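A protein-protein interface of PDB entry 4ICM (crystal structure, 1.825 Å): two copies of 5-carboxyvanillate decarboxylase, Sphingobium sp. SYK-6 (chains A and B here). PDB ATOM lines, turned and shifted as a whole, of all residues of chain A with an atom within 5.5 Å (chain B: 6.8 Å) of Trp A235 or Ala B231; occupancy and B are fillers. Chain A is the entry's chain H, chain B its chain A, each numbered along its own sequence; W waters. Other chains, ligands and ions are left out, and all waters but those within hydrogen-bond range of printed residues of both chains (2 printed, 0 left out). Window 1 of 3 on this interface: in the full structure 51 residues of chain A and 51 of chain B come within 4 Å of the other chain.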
ATOM      1  N   ALA A 231     -22.179 -34.647 -18.487  1.00  0.00           N
ATOM      2  CA  ALA A 231     -23.584 -34.200 -18.404  1.00  0.00           C
ATOM      3  C   ALA A 231     -24.293 -33.935 -19.742  1.00  0.00           C
ATOM      4  O   ALA A 231     -25.478 -33.650 -19.755  1.00  0.00           O
ATOM      5  CB  ALA A 231     -23.740 -32.993 -17.467  1.00  0.00           C
ATOM      6  N   ILE A 232     -23.570 -34.028 -20.858  1.00  0.00           N
ATOM      7  CA  ILE A 232     -24.205 -33.879 -22.170  1.00  0.00           C
ATOM      8  C   ILE A 232     -25.412 -34.805 -22.369  1.00  0.00           C
ATOM      9  O   ILE A 232     -26.423 -34.368 -22.921  1.00  0.00           O
ATOM     10  CB  ILE A 232     -23.182 -33.999 -23.331  1.00  0.00           C
ATOM     11  CG1 ILE A 232     -22.173 -32.846 -23.237  1.00  0.00           C
ATOM     12  CG2 ILE A 232     -23.893 -33.973 -24.684  1.00  0.00           C
ATOM     13  CD1 ILE A 232     -20.961 -32.999 -24.161  1.00  0.00           C
ATOM     14  N   PRO A 233     -25.343 -36.062 -21.878  1.00  0.00           N
ATOM     15  CA  PRO A 233     -26.554 -36.881 -21.997  1.00  0.00           C
ATOM     16  C   PRO A 233     -27.805 -36.229 -21.392  1.00  0.00           C
ATOM     17  O   PRO A 233     -28.903 -36.478 -21.884  1.00  0.00           O
ATOM     18  CB  PRO A 233     -26.194 -38.137 -21.195  1.00  0.00           C
ATOM     19  CG  PRO A 233     -24.714 -38.260 -21.348  1.00  0.00           C
ATOM     20  CD  PRO A 233     -24.222 -36.837 -21.290  1.00  0.00           C
ATOM     21  N   PHE A 234     -27.638 -35.410 -20.362  1.00  0.00           N
ATOM     22  CA  PHE A 234     -28.790 -34.801 -19.693  1.00  0.00           C
ATOM     23  C   PHE A 234     -29.395 -33.673 -20.513  1.00  0.00           C
ATOM     24  O   PHE A 234     -30.586 -33.397 -20.395  1.00  0.00           O
ATOM     25  CB  PHE A 234     -28.383 -34.277 -18.316  1.00  0.00           C
ATOM     26  CG  PHE A 234     -29.539 -34.092 -17.373  1.00  0.00           C
ATOM     27  CD1 PHE A 234     -30.241 -35.199 -16.910  1.00  0.00           C
ATOM     28  CD2 PHE A 234     -29.929 -32.831 -16.963  1.00  0.00           C
ATOM     29  CE1 PHE A 234     -31.313 -35.060 -16.043  1.00  0.00           C
ATOM     30  CE2 PHE A 234     -31.003 -32.660 -16.089  1.00  0.00           C
ATOM     31  CZ  PHE A 234     -31.706 -33.786 -15.627  1.00  0.00           C
ATOM     32  N   TRP A 235     -28.562 -33.022 -21.331  1.00  0.00           N
ATOM     33  CA  TRP A 235     -28.967 -31.862 -22.141  1.00  0.00           C
ATOM     34  C   TRP A 235     -29.444 -32.183 -23.560  1.00  0.00           C
ATOM     35  O   TRP A 235     -29.681 -31.259 -24.336  1.00  0.00           O
ATOM     36  CB  TRP A 235     -27.798 -30.880 -22.297  1.00  0.00           C
ATOM     37  CG  TRP A 235     -27.357 -30.153 -21.070  1.00  0.00           C
ATOM     38  CD1 TRP A 235     -26.263 -30.437 -20.288  1.00  0.00           C
ATOM     39  CD2 TRP A 235     -27.970 -28.990 -20.500  1.00  0.00           C
ATOM     40  NE1 TRP A 235     -26.176 -29.523 -19.261  1.00  0.00           N
ATOM     41  CE2 TRP A 235     -27.206 -28.625 -19.370  1.00  0.00           C
ATOM     42  CE3 TRP A 235     -29.085 -28.218 -20.842  1.00  0.00           C
ATOM     43  CZ2 TRP A 235     -27.531 -27.528 -18.569  1.00  0.00           C
ATOM     44  CZ3 TRP A 235     -29.412 -27.132 -20.042  1.00  0.00           C
ATOM     45  CH2 TRP A 235     -28.634 -26.796 -18.920  1.00  0.00           C
ATOM     46  N   LEU A 236     -29.556 -33.457 -23.928  1.00  0.00           N
ATOM     47  CA  LEU A 236     -29.816 -33.799 -25.343  1.00  0.00           C
ATOM     48  C   LEU A 236     -31.089 -33.189 -25.946  1.00  0.00           C
ATOM     49  O   LEU A 236     -31.096 -32.782 -27.116  1.00  0.00           O
ATOM     50  CB  LEU A 236     -29.838 -35.317 -25.561  1.00  0.00           C
ATOM     51  CG  LEU A 236     -28.555 -36.097 -25.275  1.00  0.00           C
ATOM     52  CD1 LEU A 236     -28.798 -37.582 -25.484  1.00  0.00           C
ATOM     53  CD2 LEU A 236     -27.415 -35.596 -26.132  1.00  0.00           C
ATOM     54  N   TRP A 237     -32.175 -33.135 -25.175  1.00  0.00           N
ATOM     55  CA  TRP A 237     -33.436 -32.692 -25.754  1.00  0.00           C
ATOM     56  C   TRP A 237     -33.354 -31.197 -26.068  1.00  0.00           C
ATOM     57  O   TRP A 237     -33.809 -30.745 -27.121  1.00  0.00           O
ATOM     58  CB  TRP A 237     -34.614 -32.979 -24.818  1.00  0.00           C
ATOM     59  CG  TRP A 237     -35.946 -32.824 -25.480  1.00  0.00           C
ATOM     60  CD1 TRP A 237     -36.664 -33.801 -26.110  1.00  0.00           C
ATOM     61  CD2 TRP A 237     -36.730 -31.620 -25.584  1.00  0.00           C
ATOM     62  NE1 TRP A 237     -37.843 -33.281 -26.603  1.00  0.00           N
ATOM     63  CE2 TRP A 237     -37.908 -31.946 -26.290  1.00  0.00           C
ATOM     64  CE3 TRP A 237     -36.545 -30.303 -25.160  1.00  0.00           C
ATOM     65  CZ2 TRP A 237     -38.895 -31.003 -26.582  1.00  0.00           C
ATOM     66  CZ3 TRP A 237     -37.523 -29.368 -25.441  1.00  0.00           C
ATOM     67  CH2 TRP A 237     -38.688 -29.720 -26.145  1.00  0.00           C
ATOM     68  N   ARG A 238     -32.755 -30.445 -25.149  1.00  0.00           N
ATOM     69  CA  ARG A 238     -32.592 -28.995 -25.301  1.00  0.00           C
ATOM     70  C   ARG A 238     -31.558 -28.649 -26.379  1.00  0.00           C
ATOM     71  O   ARG A 238     -31.740 -27.698 -27.135  1.00  0.00           O
ATOM     72  CB  ARG A 238     -32.193 -28.385 -23.956  1.00  0.00           C
ATOM     73  CG  ARG A 238     -32.077 -26.865 -23.939  1.00  0.00           C
ATOM     74  CD  ARG A 238     -32.544 -26.395 -22.589  1.00  0.00           C
ATOM     75  NE  ARG A 238     -32.213 -25.008 -22.262  1.00  0.00           N
ATOM     76  CZ  ARG A 238     -32.999 -23.969 -22.501  1.00  0.00           C
ATOM     77  NH1 ARG A 238     -34.163 -24.129 -23.131  1.00  0.00           N
ATOM     78  NH2 ARG A 238     -32.609 -22.758 -22.124  1.00  0.00           N
ATOM     79  N   LEU A 239     -30.470 -29.411 -26.451  1.00  0.00           N
ATOM     80  CA  LEU A 239     -29.532 -29.261 -27.572  1.00  0.00           C
ATOM     81  C   LEU A 239     -30.244 -29.421 -28.913  1.00  0.00           C
ATOM     82  O   LEU A 239     -30.044 -28.631 -29.839  1.00  0.00           O
ATOM     83  CB  LEU A 239     -28.400 -30.285 -27.477  1.00  0.00           C
ATOM     84  CG  LEU A 239     -27.341 -29.993 -26.421  1.00  0.00           C
ATOM     85  CD1 LEU A 239     -26.520 -31.247 -26.174  1.00  0.00           C
ATOM     86  CD2 LEU A 239     -26.436 -28.826 -26.834  1.00  0.00           C
ATOM     87  N   ASP A 240     -31.077 -30.443 -29.021  1.00  0.00           N
ATOM     88  CA  ASP A 240     -31.847 -30.648 -30.245  1.00  0.00           C
ATOM     89  C   ASP A 240     -32.872 -29.556 -30.472  1.00  0.00           C
ATOM     90  O   ASP A 240     -32.992 -29.025 -31.588  1.00  0.00           O
ATOM     91  CB  ASP A 240     -32.567 -31.994 -30.207  1.00  0.00           C
ATOM     92  CG  ASP A 240     -31.636 -33.165 -30.449  1.00  0.00           C
ATOM     93  OD1 ASP A 240     -30.473 -32.950 -30.865  1.00  0.00           O
ATOM     94  OD2 ASP A 240     -32.081 -34.308 -30.233  1.00  0.00           O
ATOM     95  N   TYR A 282     -30.320 -43.538 -16.319  1.00  0.00           N
ATOM     96  CA  TYR A 282     -30.684 -42.470 -17.251  1.00  0.00           C
ATOM     97  C   TYR A 282     -29.863 -42.573 -18.557  1.00  0.00           C
ATOM     98  O   TYR A 282     -30.396 -42.472 -19.679  1.00  0.00           O
ATOM     99  CB  TYR A 282     -30.454 -41.080 -16.630  1.00  0.00           C
ATOM    100  CG  TYR A 282     -30.663 -39.984 -17.647  1.00  0.00           C
ATOM    101  CD1 TYR A 282     -31.942 -39.514 -17.936  1.00  0.00           C
ATOM    102  CD2 TYR A 282     -29.591 -39.473 -18.382  1.00  0.00           C
ATOM    103  CE1 TYR A 282     -32.146 -38.528 -18.913  1.00  0.00           C
ATOM    104  CE2 TYR A 282     -29.779 -38.512 -19.345  1.00  0.00           C
ATOM    105  CZ  TYR A 282     -31.057 -38.040 -19.616  1.00  0.00           C
ATOM    106  OH  TYR A 282     -31.229 -37.075 -20.594  1.00  0.00           O
ATOM    107  N   ALA B 194     -29.940 -20.222 -25.500  1.00  0.00           N
ATOM    108  CA  ALA B 194     -30.501 -21.393 -24.824  1.00  0.00           C
ATOM    109  C   ALA B 194     -29.806 -22.722 -25.154  1.00  0.00           C
ATOM    110  O   ALA B 194     -29.816 -23.664 -24.345  1.00  0.00           O
ATOM    111  CB  ALA B 194     -31.998 -21.488 -25.131  1.00  0.00           C
ATOM    112  N   ILE B 195     -29.197 -22.807 -26.330  1.00  0.00           N
ATOM    113  CA  ILE B 195     -28.608 -24.075 -26.759  1.00  0.00           C
ATOM    114  C   ILE B 195     -27.436 -24.512 -25.858  1.00  0.00           C
ATOM    115  O   ILE B 195     -27.190 -25.703 -25.696  1.00  0.00           O
ATOM    116  CB  ILE B 195     -28.194 -24.041 -28.257  1.00  0.00           C
ATOM    117  CG1 ILE B 195     -28.013 -25.457 -28.816  1.00  0.00           C
ATOM    118  CG2 ILE B 195     -26.911 -23.241 -28.453  1.00  0.00           C
ATOM    119  CD1 ILE B 195     -27.790 -25.494 -30.346  1.00  0.00           C
ATOM    120  N   TRP B 196     -26.710 -23.567 -25.269  1.00  0.00           N
ATOM    121  CA  TRP B 196     -25.627 -23.964 -24.371  1.00  0.00           C
ATOM    122  C   TRP B 196     -25.254 -22.937 -23.305  1.00  0.00           C
ATOM    123  O   TRP B 196     -25.168 -23.260 -22.117  1.00  0.00           O
ATOM    124  CB  TRP B 196     -24.371 -24.397 -25.159  1.00  0.00           C
ATOM    125  CG  TRP B 196     -23.404 -25.162 -24.294  1.00  0.00           C
ATOM    126  CD1 TRP B 196     -22.148 -24.772 -23.912  1.00  0.00           C
ATOM    127  CD2 TRP B 196     -23.640 -26.429 -23.661  1.00  0.00           C
ATOM    128  NE1 TRP B 196     -21.584 -25.729 -23.088  1.00  0.00           N
ATOM    129  CE2 TRP B 196     -22.482 -26.749 -22.914  1.00  0.00           C
ATOM    130  CE3 TRP B 196     -24.719 -27.318 -23.647  1.00  0.00           C
ATOM    131  CZ2 TRP B 196     -22.373 -27.924 -22.166  1.00  0.00           C
ATOM    132  CZ3 TRP B 196     -24.613 -28.486 -22.901  1.00  0.00           C
ATOM    133  CH2 TRP B 196     -23.444 -28.780 -22.175  1.00  0.00           C
ATOM    134  N   TYR B 198     -26.774 -20.394 -21.861  1.00  0.00           N
ATOM    135  CA  TYR B 198     -27.719 -20.139 -20.768  1.00  0.00           C
ATOM    136  C   TYR B 198     -27.502 -21.100 -19.582  1.00  0.00           C
ATOM    137  O   TYR B 198     -27.390 -20.675 -18.435  1.00  0.00           O
ATOM    138  CB  TYR B 198     -29.162 -20.214 -21.276  1.00  0.00           C
ATOM    139  CG  TYR B 198     -29.646 -18.928 -21.943  1.00  0.00           C
ATOM    140  CD1 TYR B 198     -28.767 -17.883 -22.206  1.00  0.00           C
ATOM    141  CD2 TYR B 198     -30.986 -18.759 -22.294  1.00  0.00           C
ATOM    142  CE1 TYR B 198     -29.202 -16.696 -22.813  1.00  0.00           C
ATOM    143  CE2 TYR B 198     -31.435 -17.566 -22.899  1.00  0.00           C
ATOM    144  CZ  TYR B 198     -30.541 -16.555 -23.161  1.00  0.00           C
ATOM    145  OH  TYR B 198     -30.963 -15.380 -23.745  1.00  0.00           O
ATOM    146  N   GLY B 199     -27.415 -22.388 -19.874  1.00  0.00           N
ATOM    147  CA  GLY B 199     -27.326 -23.387 -18.833  1.00  0.00           C
ATOM    148  C   GLY B 199     -26.003 -23.340 -18.094  1.00  0.00           C
ATOM    149  O   GLY B 199     -25.960 -23.535 -16.875  1.00  0.00           O
ATOM    150  N   ILE B 200     -24.924 -23.084 -18.826  1.00  0.00           N
ATOM    151  CA  ILE B 200     -23.596 -23.037 -18.209  1.00  0.00           C
ATOM    152  C   ILE B 200     -23.495 -21.821 -17.277  1.00  0.00           C
ATOM    153  O   ILE B 200     -22.994 -21.921 -16.154  1.00  0.00           O
ATOM    154  CB  ILE B 200     -22.490 -22.972 -19.267  1.00  0.00           C
ATOM    155  CG1 ILE B 200     -22.473 -24.260 -20.105  1.00  0.00           C
ATOM    156  CG2 ILE B 200     -21.133 -22.745 -18.608  1.00  0.00           C
ATOM    157  CD1 ILE B 200     -22.401 -25.537 -19.289  1.00  0.00           C
ATOM    158  N   SER B 203     -26.092 -22.404 -14.147  1.00  0.00           N
ATOM    159  CA  SER B 203     -25.677 -23.470 -13.251  1.00  0.00           C
ATOM    160  C   SER B 203     -24.411 -23.090 -12.505  1.00  0.00           C
ATOM    161  O   SER B 203     -24.254 -23.441 -11.342  1.00  0.00           O
ATOM    162  CB  SER B 203     -25.463 -24.789 -13.997  1.00  0.00           C
ATOM    163  OG  SER B 203     -24.458 -24.652 -14.978  1.00  0.00           O
ATOM    164  N   GLY B 226     -34.845 -23.293 -13.741  1.00  0.00           N
ATOM    165  CA  GLY B 226     -35.548 -23.882 -14.863  1.00  0.00           C
ATOM    166  C   GLY B 226     -34.664 -24.858 -15.625  1.00  0.00           C
ATOM    167  O   GLY B 226     -33.562 -25.185 -15.180  1.00  0.00           O
ATOM    168  N   HIS B 227     -35.158 -25.323 -16.765  1.00  0.00           N
ATOM    169  CA  HIS B 227     -34.385 -26.189 -17.669  1.00  0.00           C
ATOM    170  C   HIS B 227     -33.833 -27.408 -16.951  1.00  0.00           C
ATOM    171  O   HIS B 227     -32.644 -27.729 -17.040  1.00  0.00           O
ATOM    172  CB  HIS B 227     -33.320 -25.367 -18.382  1.00  0.00           C
ATOM    173  CG  HIS B 227     -33.839 -24.035 -18.817  1.00  0.00           C
ATOM    174  ND1 HIS B 227     -33.461 -22.851 -18.217  1.00  0.00           N
ATOM    175  CD2 HIS B 227     -34.794 -23.711 -19.723  1.00  0.00           C
ATOM    176  CE1 HIS B 227     -34.131 -21.851 -18.767  1.00  0.00           C
ATOM    177  NE2 HIS B 227     -34.952 -22.345 -19.680  1.00  0.00           N
ATOM    178  N   MET B 228     -34.745 -28.059 -16.234  1.00  0.00           N
ATOM    179  CA  MET B 228     -34.472 -29.245 -15.429  1.00  0.00           C
ATOM    180  C   MET B 228     -33.298 -29.025 -14.475  1.00  0.00           C
ATOM    181  O   MET B 228     -32.421 -29.880 -14.348  1.00  0.00           O
ATOM    182  CB  MET B 228     -34.248 -30.475 -16.317  1.00  0.00           C
ATOM    183  CG  MET B 228     -34.655 -31.799 -15.676  1.00  0.00           C
ATOM    184  SD  MET B 228     -36.438 -31.941 -15.366  1.00  0.00           S
ATOM    185  CE  MET B 228     -37.029 -32.072 -17.043  1.00  0.00           C
ATOM    186  N   GLY B 229     -33.304 -27.871 -13.819  1.00  0.00           N
ATOM    187  CA  GLY B 229     -32.313 -27.519 -12.808  1.00  0.00           C
ATOM    188  C   GLY B 229     -30.958 -27.144 -13.385  1.00  0.00           C
ATOM    189  O   GLY B 229     -29.943 -27.235 -12.692  1.00  0.00           O
ATOM    190  N   GLU B 230     -30.949 -26.702 -14.640  1.00  0.00           N
ATOM    191  CA  GLU B 230     -29.716 -26.384 -15.369  1.00  0.00           C
ATOM    192  C   GLU B 230     -28.660 -27.489 -15.241  1.00  0.00           C
ATOM    193  O   GLU B 230     -27.462 -27.225 -15.100  1.00  0.00           O
ATOM    194  CB  GLU B 230     -29.192 -24.996 -14.971  1.00  0.00           C
ATOM    195  CG  GLU B 230     -30.299 -23.910 -14.955  1.00  0.00           C
ATOM    196  CD  GLU B 230     -30.769 -23.450 -16.355  1.00  0.00           C
ATOM    197  OE1 GLU B 230     -30.259 -23.950 -17.384  1.00  0.00           O
ATOM    198  OE2 GLU B 230     -31.662 -22.575 -16.427  1.00  0.00           O
ATOM    199  N   ALA B 231     -29.147 -28.730 -15.257  1.00  0.00           N
ATOM    200  CA  ALA B 231     -28.351 -29.966 -15.160  1.00  0.00           C
ATOM    201  C   ALA B 231     -27.695 -30.232 -13.794  1.00  0.00           C
ATOM    202  O   ALA B 231     -27.082 -31.279 -13.601  1.00  0.00           O
ATOM    203  CB  ALA B 231     -27.303 -30.045 -16.267  1.00  0.00           C
ATOM    204  N   ILE B 232     -27.809 -29.300 -12.857  1.00  0.00           N
ATOM    205  CA  ILE B 232     -27.293 -29.560 -11.492  1.00  0.00           C
ATOM    206  C   ILE B 232     -27.780 -30.910 -10.900  1.00  0.00           C
ATOM    207  O   ILE B 232     -26.977 -31.647 -10.303  1.00  0.00           O
ATOM    208  CB  ILE B 232     -27.507 -28.364 -10.527  1.00  0.00           C
ATOM    209  CG1 ILE B 232     -26.732 -27.142 -11.033  1.00  0.00           C
ATOM    210  CG2 ILE B 232     -27.011 -28.711  -9.121  1.00  0.00           C
ATOM    211  CD1 ILE B 232     -26.944 -25.902 -10.210  1.00  0.00           C
ATOM    212  N   PRO B 233     -29.067 -31.270 -11.113  1.00  0.00           N
ATOM    213  CA  PRO B 233     -29.510 -32.585 -10.624  1.00  0.00           C
ATOM    214  C   PRO B 233     -28.667 -33.748 -11.138  1.00  0.00           C
ATOM    215  O   PRO B 233     -28.548 -34.769 -10.444  1.00  0.00           O
ATOM    216  CB  PRO B 233     -30.952 -32.683 -11.162  1.00  0.00           C
ATOM    217  CG  PRO B 233     -31.421 -31.263 -11.154  1.00  0.00           C
ATOM    218  CD  PRO B 233     -30.207 -30.481 -11.631  1.00  0.00           C
ATOM    219  N   PHE B 234     -28.090 -33.604 -12.328  1.00  0.00           N
ATOM    220  CA  PHE B 234     -27.293 -34.680 -12.898  1.00  0.00           C
ATOM    221  C   PHE B 234     -25.917 -34.810 -12.256  1.00  0.00           C
ATOM    222  O   PHE B 234     -25.345 -35.907 -12.241  1.00  0.00           O
ATOM    223  CB  PHE B 234     -27.138 -34.501 -14.411  1.00  0.00           C
ATOM    224  CG  PHE B 234     -26.799 -35.773 -15.133  1.00  0.00           C
ATOM    225  CD1 PHE B 234     -27.702 -36.833 -15.156  1.00  0.00           C
ATOM    226  CD2 PHE B 234     -25.591 -35.908 -15.798  1.00  0.00           C
ATOM    227  CE1 PHE B 234     -27.398 -38.017 -15.831  1.00  0.00           C
ATOM    228  CE2 PHE B 234     -25.274 -37.096 -16.476  1.00  0.00           C
ATOM    229  CZ  PHE B 234     -26.181 -38.141 -16.489  1.00  0.00           C
ATOM    230  N   TRP B 235     -25.403 -33.701 -11.729  1.00  0.00           N
ATOM    231  CA  TRP B 235     -24.037 -33.628 -11.192  1.00  0.00           C
ATOM    232  C   TRP B 235     -23.937 -33.841  -9.686  1.00  0.00           C
ATOM    233  O   TRP B 235     -22.852 -33.663  -9.125  1.00  0.00           O
ATOM    234  CB  TRP B 235     -23.427 -32.241 -11.457  1.00  0.00           C
ATOM    235  CG  TRP B 235     -23.032 -31.951 -12.855  1.00  0.00           C
ATOM    236  CD1 TRP B 235     -23.716 -31.186 -13.752  1.00  0.00           C
ATOM    237  CD2 TRP B 235     -21.842 -32.393 -13.524  1.00  0.00           C
ATOM    238  NE1 TRP B 235     -23.033 -31.135 -14.944  1.00  0.00           N
ATOM    239  CE2 TRP B 235     -21.881 -31.872 -14.830  1.00  0.00           C
ATOM    240  CE3 TRP B 235     -20.751 -33.187 -13.144  1.00  0.00           C
ATOM    241  CZ2 TRP B 235     -20.872 -32.112 -15.768  1.00  0.00           C
ATOM    242  CZ3 TRP B 235     -19.745 -33.427 -14.079  1.00  0.00           C
ATOM    243  CH2 TRP B 235     -19.819 -32.895 -15.380  1.00  0.00           C
ATOM    244  N   LEU B 236     -25.041 -34.202  -9.027  1.00  0.00           N
ATOM    245  CA  LEU B 236     -25.071 -34.203  -7.556  1.00  0.00           C
ATOM    246  C   LEU B 236     -24.031 -35.106  -6.920  1.00  0.00           C
ATOM    247  O   LEU B 236     -23.431 -34.736  -5.920  1.00  0.00           O
ATOM    248  CB  LEU B 236     -26.454 -34.590  -7.013  1.00  0.00           C
ATOM    249  CG  LEU B 236     -27.630 -33.629  -7.230  1.00  0.00           C
ATOM    250  CD1 LEU B 236     -28.879 -34.157  -6.505  1.00  0.00           C
ATOM    251  CD2 LEU B 236     -27.314 -32.226  -6.747  1.00  0.00           C
ATOM    252  N   PHE B 263     -28.910 -28.615  -2.285  1.00  0.00           N
ATOM    253  CA  PHE B 263     -29.701 -28.558  -3.510  1.00  0.00           C
ATOM    254  C   PHE B 263     -31.116 -29.029  -3.224  1.00  0.00           C
ATOM    255  O   PHE B 263     -32.074 -28.401  -3.645  1.00  0.00           O
ATOM    256  CB  PHE B 263     -29.092 -29.323  -4.690  1.00  0.00           C
ATOM    257  CG  PHE B 263     -29.709 -28.929  -6.000  1.00  0.00           C
ATOM    258  CD1 PHE B 263     -29.366 -27.722  -6.597  1.00  0.00           C
ATOM    259  CD2 PHE B 263     -30.702 -29.697  -6.576  1.00  0.00           C
ATOM    260  CE1 PHE B 263     -29.954 -27.330  -7.782  1.00  0.00           C
ATOM    261  CE2 PHE B 263     -31.307 -29.300  -7.758  1.00  0.00           C
ATOM    262  CZ  PHE B 263     -30.928 -28.122  -8.364  1.00  0.00           C
ATOM    263  N   VAL B 274     -37.156 -28.613 -21.361  1.00  0.00           N
ATOM    264  CA  VAL B 274     -36.624 -29.974 -21.275  1.00  0.00           C
ATOM    265  C   VAL B 274     -37.788 -30.950 -21.196  1.00  0.00           C
ATOM    266  O   VAL B 274     -38.124 -31.470 -20.124  1.00  0.00           O
ATOM    267  CB  VAL B 274     -35.689 -30.186 -20.049  1.00  0.00           C
ATOM    268  CG1 VAL B 274     -35.093 -31.588 -20.062  1.00  0.00           C
ATOM    269  CG2 VAL B 274     -34.557 -29.152 -20.040  1.00  0.00           C
ATOM    270  N   TYR B 282     -35.645 -39.072 -13.895  1.00  0.00           N
ATOM    271  CA  TYR B 282     -34.377 -38.954 -13.179  1.00  0.00           C
ATOM    272  C   TYR B 282     -34.480 -37.910 -12.061  1.00  0.00           C
ATOM    273  O   TYR B 282     -34.059 -38.142 -10.910  1.00  0.00           O
ATOM    274  CB  TYR B 282     -33.243 -38.581 -14.135  1.00  0.00           C
ATOM    275  CG  TYR B 282     -31.976 -38.251 -13.372  1.00  0.00           C
ATOM    276  CD1 TYR B 282     -31.106 -39.260 -12.954  1.00  0.00           C
ATOM    277  CD2 TYR B 282     -31.674 -36.942 -13.018  1.00  0.00           C
ATOM    278  CE1 TYR B 282     -29.961 -38.965 -12.206  1.00  0.00           C
ATOM    279  CE2 TYR B 282     -30.531 -36.645 -12.276  1.00  0.00           C
ATOM    280  CZ  TYR B 282     -29.681 -37.651 -11.881  1.00  0.00           C
ATOM    281  OH  TYR B 282     -28.550 -37.343 -11.145  1.00  0.00           O
HETATM  282  O   HOH W   1     -30.649 -23.255 -20.056  1.00  0.00           O
HETATM  283  O   HOH W   2     -23.976 -29.483 -17.188  1.00  0.00           O
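The guanidinium group of Arg A238 sits at hydrogen-bond distance from the backbone carbonyl oxygen of Ala B194 (3.4 Å). A ring nitrogen (NE2) of His B227 sits close to the guanidinium group (NH2) of Arg A238 (3.4 Å).
Among the printed residues, 16 pairs touch across the chains. Among the printed residues, no Asp or Glu carboxylate lies within 4 Å of a Lys or Arg side-chain nitrogen of the other chain.
Water W1 lies within hydrogen-bond range of the side-chain carboxylate of Glu B230 (2.8 Å), the guanidinium group of Arg A238 (2.9 Å), the backbone NH of Gly B199 (3.4 Å) and a ring nitrogen (ND1) of His B227 (3.4 Å). Water W2 bridges NE1 of Trp B235 and NE1 of Trp A235.
Among the printed residues, merely in contact across the chains: Ala A231 with Trp B235 (3.2 Å), Trp A235 with Ala B231 (3.2 Å), Leu A239 with Ile B195 (3.4 Å), Trp A235 with Glu B230 (3.5 Å), Phe A234 with Phe B234 (3.5 Å), Phe A234 with Met B228 (3.6 Å), Phe A234 with Tyr B282 (3.6 Å), Trp A235 with Gly B199 (3.7 Å), Trp A235 with Trp B196 (3.7 Å), Tyr A282 with Phe B234 (3.7 Å), Ala A231 with Phe B234 (3.7 Å), Phe A234 with Ala B231 (3.7 Å), Trp A237 with Val B274 (3.9 Å) and Leu A239 with Trp B196 (3.9 Å).
Ala A231 touches Phe B234, and with the chains exchanged Phe A234 touches Ala B231. Ala A231 touches Trp B235, and with the chains exchanged Trp A235 touches Ala B231. Phe B234 touches its own counterpart, Phe A234. Phe A234 touches Tyr B282, and with the chains exchanged Tyr A282 touches Phe B234. 7 positions are printed for both chains. Of the 16 pairs that touch across the chains among the printed residues, 7 have their exchanged pair printed and touching as well.
Of the printed residues of chain B, Trp A235 touches Trp B196, Gly B199, Glu B230 and Ala B231. Of the printed residues of chain A, Val B274 touches Trp A237 (3.9 Å). Of the printed residues of chain A, Gly B199 touches Trp A235 (3.7 Å). Printed residues of chain B within 4 Å of Phe A234: Met B228 (3.6 Å), Ala B231 (3.7 Å), Phe B234 (3.5 Å) and Tyr B282 (3.6 Å). Of the printed residues of chain A, Ile B195 touches Leu A239 (3.4 Å). Gly B229 touches none of the printed residues of chain A. The nearest residue of chain B that does not touch Trp A235 is His B227 (4.5 Å). The nearest residue of chain A that does not touch Ala B231 is Ala A231 (4.8 Å).
The backbone carbonyl oxygen (O) of Gly B199 sits at hydrogen-bond distance from the side-chain hydroxyl (OG) of Ser B203 (2.7 Å). OE2 of Glu B230 lies within hydrogen-bond range of ND1 of His B227. The backbone carbonyl oxygen (O) of Pro B233 sits at hydrogen-bond distance from the side-chain hydroxyl (OH) of Tyr B282, at 2.7 Å. The backbone carbonyl oxygen (O) of Pro A233 sits at hydrogen-bond distance from the side-chain hydroxyl (OH) of Tyr A282.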
